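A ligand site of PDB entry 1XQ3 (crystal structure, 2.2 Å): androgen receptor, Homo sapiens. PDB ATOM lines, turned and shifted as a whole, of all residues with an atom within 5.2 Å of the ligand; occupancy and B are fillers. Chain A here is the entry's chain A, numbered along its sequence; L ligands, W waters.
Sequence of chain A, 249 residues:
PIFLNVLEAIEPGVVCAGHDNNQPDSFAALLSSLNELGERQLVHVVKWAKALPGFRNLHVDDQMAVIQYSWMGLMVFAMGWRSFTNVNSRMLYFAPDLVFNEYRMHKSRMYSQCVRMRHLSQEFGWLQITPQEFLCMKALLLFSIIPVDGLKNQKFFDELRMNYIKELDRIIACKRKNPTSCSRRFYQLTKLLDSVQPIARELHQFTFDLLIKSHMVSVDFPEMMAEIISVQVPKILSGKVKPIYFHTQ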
ATOM      1  N   LEU A  31      10.239  32.007  -9.043  1.00  0.00           N
ATOM      2  CA  LEU A  31      10.693  30.986  -9.986  1.00  0.00           C
ATOM      3  C   LEU A  31      12.011  31.384 -10.665  1.00  0.00           C
ATOM      4  O   LEU A  31      12.870  30.542 -10.921  1.00  0.00           O
ATOM      5  CB  LEU A  31       9.607  30.704 -11.021  1.00  0.00           C
ATOM      6  CG  LEU A  31       8.390  29.886 -10.551  1.00  0.00           C
ATOM      7  CD1 LEU A  31       8.743  28.423 -10.486  1.00  0.00           C
ATOM      8  CD2 LEU A  31       7.933  30.353  -9.189  1.00  0.00           C
ATOM      9  N   LEU A  34      14.636  30.620  -8.178  1.00  0.00           N
ATOM     10  CA  LEU A  34      14.848  29.174  -8.105  1.00  0.00           C
ATOM     11  C   LEU A  34      15.672  28.721  -9.294  1.00  0.00           C
ATOM     12  O   LEU A  34      16.572  27.895  -9.134  1.00  0.00           O
ATOM     13  CB  LEU A  34      13.499  28.427  -8.084  1.00  0.00           C
ATOM     14  CG  LEU A  34      12.779  28.426  -6.726  1.00  0.00           C
ATOM     15  CD1 LEU A  34      11.413  27.784  -6.875  1.00  0.00           C
ATOM     16  CD2 LEU A  34      13.621  27.667  -5.693  1.00  0.00           C
ATOM     17  N   ASN A  35      15.372  29.274 -10.473  1.00  0.00           N
ATOM     18  CA  ASN A  35      16.119  28.904 -11.676  1.00  0.00           C
ATOM     19  C   ASN A  35      17.563  29.326 -11.570  1.00  0.00           C
ATOM     20  O   ASN A  35      18.460  28.606 -12.013  1.00  0.00           O
ATOM     21  CB  ASN A  35      15.479  29.494 -12.937  1.00  0.00           C
ATOM     22  CG  ASN A  35      14.243  28.727 -13.365  1.00  0.00           C
ATOM     23  OD1 ASN A  35      14.018  27.608 -12.891  1.00  0.00           O
ATOM     24  ND2 ASN A  35      13.452  29.298 -14.275  1.00  0.00           N
ATOM     25  N   LEU A  37      19.191  29.630  -8.806  1.00  0.00           N
ATOM     26  CA  LEU A  37      19.746  28.702  -7.823  1.00  0.00           C
ATOM     27  C   LEU A  37      20.003  27.356  -8.482  1.00  0.00           C
ATOM     28  O   LEU A  37      21.008  26.698  -8.215  1.00  0.00           O
ATOM     29  CB  LEU A  37      18.771  28.523  -6.655  1.00  0.00           C
ATOM     30  CG  LEU A  37      19.291  27.578  -5.558  1.00  0.00           C
ATOM     31  CD1 LEU A  37      20.597  28.119  -4.990  1.00  0.00           C
ATOM     32  CD2 LEU A  37      18.248  27.433  -4.461  1.00  0.00           C
ATOM     33  N   GLY A  38      19.083  26.941  -9.347  1.00  0.00           N
ATOM     34  CA  GLY A  38      19.250  25.682 -10.038  1.00  0.00           C
ATOM     35  C   GLY A  38      20.527  25.678 -10.859  1.00  0.00           C
ATOM     36  O   GLY A  38      21.289  24.714 -10.840  1.00  0.00           O
ATOM     37  N   GLN A  41      23.485  25.464  -8.464  1.00  0.00           N
ATOM     38  CA  GLN A  41      23.633  24.151  -7.882  1.00  0.00           C
ATOM     39  C   GLN A  41      24.142  23.172  -8.919  1.00  0.00           C
ATOM     40  O   GLN A  41      24.897  22.246  -8.602  1.00  0.00           O
ATOM     41  CB  GLN A  41      22.311  23.669  -7.285  1.00  0.00           C
ATOM     42  CG  GLN A  41      21.936  24.380  -5.988  1.00  0.00           C
ATOM     43  CD  GLN A  41      20.938  23.588  -5.155  1.00  0.00           C
ATOM     44  OE1 GLN A  41      20.522  24.008  -4.068  1.00  0.00           O
ATOM     45  NE2 GLN A  41      20.555  22.416  -5.672  1.00  0.00           N
ATOM     46  N   TRP A  71      20.102  15.265 -12.101  1.00  0.00           N
ATOM     47  CA  TRP A  71      20.156  16.604 -11.551  1.00  0.00           C
ATOM     48  C   TRP A  71      18.959  16.988 -10.679  1.00  0.00           C
ATOM     49  O   TRP A  71      19.130  17.386  -9.526  1.00  0.00           O
ATOM     50  CB  TRP A  71      20.342  17.609 -12.695  1.00  0.00           C
ATOM     51  CG  TRP A  71      20.173  19.057 -12.351  1.00  0.00           C
ATOM     52  CD1 TRP A  71      20.940  19.816 -11.493  1.00  0.00           C
ATOM     53  CD2 TRP A  71      19.185  19.953 -12.895  1.00  0.00           C
ATOM     54  NE1 TRP A  71      20.494  21.116 -11.480  1.00  0.00           N
ATOM     55  CE2 TRP A  71      19.429  21.233 -12.325  1.00  0.00           C
ATOM     56  CE3 TRP A  71      18.140  19.805 -13.810  1.00  0.00           C
ATOM     57  CZ2 TRP A  71      18.640  22.356 -12.645  1.00  0.00           C
ATOM     58  CZ3 TRP A  71      17.352  20.914 -14.128  1.00  0.00           C
ATOM     59  CH2 TRP A  71      17.620  22.176 -13.550  1.00  0.00           C
ATOM     60  N   MET A  72      17.744  16.866 -11.224  1.00  0.00           N
ATOM     61  CA  MET A  72      16.543  17.234 -10.472  1.00  0.00           C
ATOM     62  C   MET A  72      16.369  16.452  -9.166  1.00  0.00           C
ATOM     63  O   MET A  72      16.125  17.042  -8.113  1.00  0.00           O
ATOM     64  CB  MET A  72      15.290  17.061 -11.319  1.00  0.00           C
ATOM     65  CG  MET A  72      14.024  17.539 -10.609  1.00  0.00           C
ATOM     66  SD  MET A  72      14.010  19.351 -10.382  1.00  0.00           S
ATOM     67  CE  MET A  72      13.662  19.868 -12.074  1.00  0.00           C
ATOM     68  N   MET A  75      19.032  17.488  -6.587  1.00  0.00           N
ATOM     69  CA  MET A  75      18.718  18.761  -5.951  1.00  0.00           C
ATOM     70  C   MET A  75      17.601  18.586  -4.918  1.00  0.00           C
ATOM     71  O   MET A  75      17.676  19.128  -3.805  1.00  0.00           O
ATOM     72  CB  MET A  75      18.282  19.808  -6.983  1.00  0.00           C
ATOM     73  CG  MET A  75      19.397  20.413  -7.852  1.00  0.00           C
ATOM     74  SD  MET A  75      18.809  21.940  -8.671  1.00  0.00           S
ATOM     75  CE  MET A  75      17.427  21.257  -9.659  1.00  0.00           C
ATOM     76  N   VAL A  76      16.570  17.827  -5.272  1.00  0.00           N
ATOM     77  CA  VAL A  76      15.448  17.582  -4.382  1.00  0.00           C
ATOM     78  C   VAL A  76      15.883  16.868  -3.103  1.00  0.00           C
ATOM     79  O   VAL A  76      15.510  17.266  -2.003  1.00  0.00           O
ATOM     80  CB  VAL A  76      14.346  16.747  -5.090  1.00  0.00           C
ATOM     81  CG1 VAL A  76      13.379  16.170  -4.066  1.00  0.00           C
ATOM     82  CG2 VAL A  76      13.579  17.621  -6.065  1.00  0.00           C
ATOM     83  N   MET A  79      18.043  19.106  -0.882  1.00  0.00           N
ATOM     84  CA  MET A  79      17.190  20.164  -0.357  1.00  0.00           C
ATOM     85  C   MET A  79      16.371  19.664   0.827  1.00  0.00           C
ATOM     86  O   MET A  79      16.274  20.336   1.852  1.00  0.00           O
ATOM     87  CB  MET A  79      16.274  20.706  -1.457  1.00  0.00           C
ATOM     88  CG  MET A  79      15.488  21.951  -1.070  1.00  0.00           C
ATOM     89  SD  MET A  79      13.964  21.593  -0.157  1.00  0.00           S
ATOM     90  CE  MET A  79      12.940  21.004  -1.502  1.00  0.00           C
ATOM     91  N   ARG A  82      18.592  19.510   3.768  1.00  0.00           N
ATOM     92  CA  ARG A  82      18.902  20.830   4.319  1.00  0.00           C
ATOM     93  C   ARG A  82      17.711  21.340   5.110  1.00  0.00           C
ATOM     94  O   ARG A  82      17.872  21.981   6.154  1.00  0.00           O
ATOM     95  CB  ARG A  82      19.225  21.846   3.221  1.00  0.00           C
ATOM     96  CG  ARG A  82      20.562  21.643   2.530  1.00  0.00           C
ATOM     97  CD  ARG A  82      20.952  22.896   1.764  1.00  0.00           C
ATOM     98  NE  ARG A  82      19.958  23.241   0.746  1.00  0.00           N
ATOM     99  CZ  ARG A  82      19.817  22.602  -0.404  1.00  0.00           C
ATOM    100  NH1 ARG A  82      20.607  21.575  -0.709  1.00  0.00           N
ATOM    101  NH2 ARG A  82      18.869  22.973  -1.258  1.00  0.00           N
ATOM    102  N   PHE A  94      15.483  25.858   0.352  1.00  0.00           N
ATOM    103  CA  PHE A  94      16.161  25.806  -0.945  1.00  0.00           C
ATOM    104  C   PHE A  94      17.563  26.391  -0.818  1.00  0.00           C
ATOM    105  O   PHE A  94      18.537  25.834  -1.333  1.00  0.00           O
ATOM    106  CB  PHE A  94      15.357  26.598  -1.971  1.00  0.00           C
ATOM    107  CG  PHE A  94      14.090  25.931  -2.377  1.00  0.00           C
ATOM    108  CD1 PHE A  94      14.110  24.818  -3.217  1.00  0.00           C
ATOM    109  CD2 PHE A  94      12.868  26.389  -1.899  1.00  0.00           C
ATOM    110  CE1 PHE A  94      12.938  24.161  -3.569  1.00  0.00           C
ATOM    111  CE2 PHE A  94      11.676  25.738  -2.239  1.00  0.00           C
ATOM    112  CZ  PHE A  94      11.712  24.626  -3.086  1.00  0.00           C
ATOM    113  N   MET A 110       3.503  26.117  -7.063  1.00  0.00           N
ATOM    114  CA  MET A 110       4.113  24.794  -6.931  1.00  0.00           C
ATOM    115  C   MET A 110       3.694  24.142  -5.617  1.00  0.00           C
ATOM    116  O   MET A 110       4.339  23.205  -5.143  1.00  0.00           O
ATOM    117  CB  MET A 110       5.643  24.905  -6.907  1.00  0.00           C
ATOM    118  CG  MET A 110       6.333  25.029  -8.234  1.00  0.00           C
ATOM    119  SD  MET A 110       8.097  24.716  -8.009  1.00  0.00           S
ATOM    120  CE  MET A 110       8.615  26.257  -7.337  1.00  0.00           C
ATOM    121  N   MET A 117       7.648  17.557  -1.560  1.00  0.00           N
ATOM    122  CA  MET A 117       9.034  17.686  -1.132  1.00  0.00           C
ATOM    123  C   MET A 117       9.140  17.832   0.378  1.00  0.00           C
ATOM    124  O   MET A 117      10.094  17.321   0.983  1.00  0.00           O
ATOM    125  CB  MET A 117       9.704  18.874  -1.828  1.00  0.00           C
ATOM    126  CG  MET A 117       9.853  18.709  -3.337  1.00  0.00           C
ATOM    127  SD  MET A 117      10.745  20.089  -4.095  1.00  0.00           S
ATOM    128  CE  MET A 117       9.400  21.124  -4.630  1.00  0.00           C
ATOM    129  N   LEU A 203       8.382  17.536 -11.024  1.00  0.00           N
ATOM    130  CA  LEU A 203       9.158  18.753 -11.202  1.00  0.00           C
ATOM    131  C   LEU A 203       9.674  18.846 -12.642  1.00  0.00           C
ATOM    132  O   LEU A 203       9.759  19.926 -13.205  1.00  0.00           O
ATOM    133  CB  LEU A 203      10.305  18.810 -10.180  1.00  0.00           C
ATOM    134  CG  LEU A 203       9.783  18.888  -8.740  1.00  0.00           C
ATOM    135  CD1 LEU A 203      10.894  18.595  -7.733  1.00  0.00           C
ATOM    136  CD2 LEU A 203       9.168  20.258  -8.504  1.00  0.00           C
ATOM    137  N   PHE A 206       6.841  20.077 -14.544  1.00  0.00           N
ATOM    138  CA  PHE A 206       6.602  21.474 -14.208  1.00  0.00           C
ATOM    139  C   PHE A 206       7.646  22.417 -14.800  1.00  0.00           C
ATOM    140  O   PHE A 206       7.282  23.413 -15.408  1.00  0.00           O
ATOM    141  CB  PHE A 206       6.527  21.634 -12.682  1.00  0.00           C
ATOM    142  CG  PHE A 206       6.171  23.021 -12.235  1.00  0.00           C
ATOM    143  CD1 PHE A 206       7.140  24.016 -12.168  1.00  0.00           C
ATOM    144  CD2 PHE A 206       4.861  23.345 -11.900  1.00  0.00           C
ATOM    145  CE1 PHE A 206       6.809  25.320 -11.775  1.00  0.00           C
ATOM    146  CE2 PHE A 206       4.508  24.653 -11.512  1.00  0.00           C
ATOM    147  CZ  PHE A 206       5.483  25.640 -11.450  1.00  0.00           C
ATOM    148  N   THR A 207       8.926  22.113 -14.648  1.00  0.00           N
ATOM    149  CA  THR A 207       9.935  23.016 -15.193  1.00  0.00           C
ATOM    150  C   THR A 207       9.878  23.043 -16.734  1.00  0.00           C
ATOM    151  O   THR A 207      10.108  24.077 -17.359  1.00  0.00           O
ATOM    152  CB  THR A 207      11.364  22.634 -14.708  1.00  0.00           C
ATOM    153  OG1 THR A 207      12.242  23.750 -14.905  1.00  0.00           O
ATOM    154  CG2 THR A 207      11.895  21.435 -15.477  1.00  0.00           C
ATOM    155  N   LEU A 210       7.082  25.226 -17.746  1.00  0.00           N
ATOM    156  CA  LEU A 210       7.484  26.577 -17.400  1.00  0.00           C
ATOM    157  C   LEU A 210       8.407  27.159 -18.470  1.00  0.00           C
ATOM    158  O   LEU A 210       8.223  28.303 -18.894  1.00  0.00           O
ATOM    159  CB  LEU A 210       8.178  26.587 -16.036  1.00  0.00           C
ATOM    160  CG  LEU A 210       8.506  27.936 -15.390  1.00  0.00           C
ATOM    161  CD1 LEU A 210       7.257  28.828 -15.343  1.00  0.00           C
ATOM    162  CD2 LEU A 210       9.044  27.694 -13.975  1.00  0.00           C
ATOM    163  N   PHE A 221      15.276  31.707 -17.545  1.00  0.00           N
ATOM    164  CA  PHE A 221      15.966  30.422 -17.398  1.00  0.00           C
ATOM    165  C   PHE A 221      17.429  30.563 -17.802  1.00  0.00           C
ATOM    166  O   PHE A 221      17.733  30.875 -18.955  1.00  0.00           O
ATOM    167  CB  PHE A 221      15.323  29.356 -18.288  1.00  0.00           C
ATOM    168  CG  PHE A 221      14.087  28.720 -17.725  1.00  0.00           C
ATOM    169  CD1 PHE A 221      12.869  29.408 -17.728  1.00  0.00           C
ATOM    170  CD2 PHE A 221      14.136  27.440 -17.203  1.00  0.00           C
ATOM    171  CE1 PHE A 221      11.714  28.811 -17.208  1.00  0.00           C
ATOM    172  CE2 PHE A 221      12.981  26.829 -16.681  1.00  0.00           C
ATOM    173  CZ  PHE A 221      11.776  27.525 -16.685  1.00  0.00           C
ATOM    174  N   MET A 225      20.649  25.461 -17.811  1.00  0.00           N
ATOM    175  CA  MET A 225      19.391  24.855 -17.392  1.00  0.00           C
ATOM    176  C   MET A 225      18.411  24.797 -18.542  1.00  0.00           C
ATOM    177  O   MET A 225      17.711  23.804 -18.729  1.00  0.00           O
ATOM    178  CB  MET A 225      18.769  25.643 -16.255  1.00  0.00           C
ATOM    179  CG  MET A 225      19.222  25.179 -14.889  1.00  0.00           C
ATOM    180  SD  MET A 225      18.296  26.025 -13.634  1.00  0.00           S
ATOM    181  CE  MET A 225      16.651  26.167 -14.481  1.00  0.00           C
ATOM    182  N   ILE A 229      16.789  21.328 -19.728  1.00  0.00           N
ATOM    183  CA  ILE A 229      15.347  21.175 -19.708  1.00  0.00           C
ATOM    184  C   ILE A 229      14.778  20.979 -21.103  1.00  0.00           C
ATOM    185  O   ILE A 229      13.772  20.303 -21.277  1.00  0.00           O
ATOM    186  CB  ILE A 229      14.684  22.386 -19.018  1.00  0.00           C
ATOM    187  CG1 ILE A 229      15.110  22.428 -17.545  1.00  0.00           C
ATOM    188  CG2 ILE A 229      13.163  22.321 -19.141  1.00  0.00           C
ATOM    189  CD1 ILE A 229      14.596  23.630 -16.765  1.00  0.00           C
HETATM  190  C1  LIG L   1      16.772  24.669  -6.703  1.00  0.00           C
HETATM  191  C2  LIG L   1      17.783  23.980  -5.802  1.00  0.00           C
HETATM  192  C3  LIG L   1      17.141  23.079  -4.744  1.00  0.00           C
HETATM  193  C4  LIG L   1      16.008  22.263  -5.186  1.00  0.00           C
HETATM  194  C5  LIG L   1      15.281  22.553  -6.322  1.00  0.00           C
HETATM  195  C6  LIG L   1      14.110  21.622  -6.730  1.00  0.00           C
HETATM  196  C7  LIG L   1      13.036  22.401  -7.501  1.00  0.00           C
HETATM  197  C8  LIG L   1      13.688  23.074  -8.773  1.00  0.00           C
HETATM  198  C9  LIG L   1      14.867  24.022  -8.345  1.00  0.00           C
HETATM  199  C10 LIG L   1      15.587  23.770  -7.191  1.00  0.00           C
HETATM  200  C11 LIG L   1      15.143  25.186  -9.264  1.00  0.00           C
HETATM  201  C12 LIG L   1      14.439  25.441 -10.407  1.00  0.00           C
HETATM  202  C13 LIG L   1      13.246  24.562 -10.850  1.00  0.00           C
HETATM  203  C14 LIG L   1      12.643  23.879  -9.578  1.00  0.00           C
HETATM  204  C15 LIG L   1      11.416  23.104 -10.128  1.00  0.00           C
HETATM  205  C16 LIG L   1      10.957  24.007 -11.308  1.00  0.00           C
HETATM  206  C17 LIG L   1      11.947  25.224 -11.371  1.00  0.00           C
HETATM  207  C18 LIG L   1      13.787  23.456 -11.848  1.00  0.00           C
HETATM  208  C19 LIG L   1      11.415  26.345 -10.486  1.00  0.00           C
HETATM  209  O1  LIG L   1      17.564  23.026  -3.614  1.00  0.00           O
HETATM  210  O2  LIG L   1      12.041  25.678 -12.706  1.00  0.00           O
HETATM  211  O   HOH W   1      19.803  20.945  -3.484  1.00  0.00           O
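An oxygen (O1) of the ligand is in hydrogen-bond range of the guanidinium group of Arg 82 (2.7 Å).
The side-chain amide oxygen (OD1) of Asn 35 lies within hydrogen-bond range of an oxygen (O2) of the ligand (2.8 Å).
The side-chain hydroxyl (OG1) of Thr 207 is in hydrogen-bond range of an oxygen (O2) of the ligand, at 2.9 Å.
An oxygen (O1) of the ligand sits close to the side-chain amide oxygen of Gln 41 (3.1 Å).
NH2 of Arg 82 is in hydrogen-bond range of OE1 of Gln 41 (3.4 Å).
The guanidinium group (NH2) of Arg 82 is in hydrogen-bond range of the backbone carbonyl oxygen (O) of Phe 94, 2.9 Å away.
SD of Met 75 lies close to NE2 of Gln 41, at 3.5 Å.
NE1 of Trp 71 lies within hydrogen-bond range of SD of Met 75, at 3.4 Å.
Leu 31 touches the ligand.
O of Leu 34 touches C11 of the ligand (3.1 Å).
Leu 37 touches the ligand.
CE of Met 72 touches C18 of the ligand (3.6 Å).
SD of Met 75 touches C2 of the ligand, at 3.7 Å.
Met 79 touches the ligand (CB to O1, 3.4 Å).
Phe 94 touches the ligand.
Leu 203 touches the ligand.
Phe 206 touches the ligand.
CD2 of Leu 210 touches O2 of the ligand, at 3.8 Å.
Hydrophobic or aromatic side chains that line the ligand: Leu 31, Leu 34, Leu 37, Met 72, Met 75, Met 79, Phe 94, Leu 203, Phe 206 and Leu 210.
Within 4 Å of the ligand: Leu 31, Leu 34, Asn 35, Leu 37, Gln 41, Met 72, Met 75, Met 79, Arg 82, Phe 94, Leu 203, Phe 206, Thr 207 and Leu 210.
Water W1 lies within hydrogen-bond range of the side-chain amide nitrogen of Gln 41 (2.7 Å), the backbone carbonyl oxygen of Met 75 (2.8 Å), the guanidinium group of Arg 82 (3.0 Å) and an oxygen (O1) of the ligand (3.1 Å).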
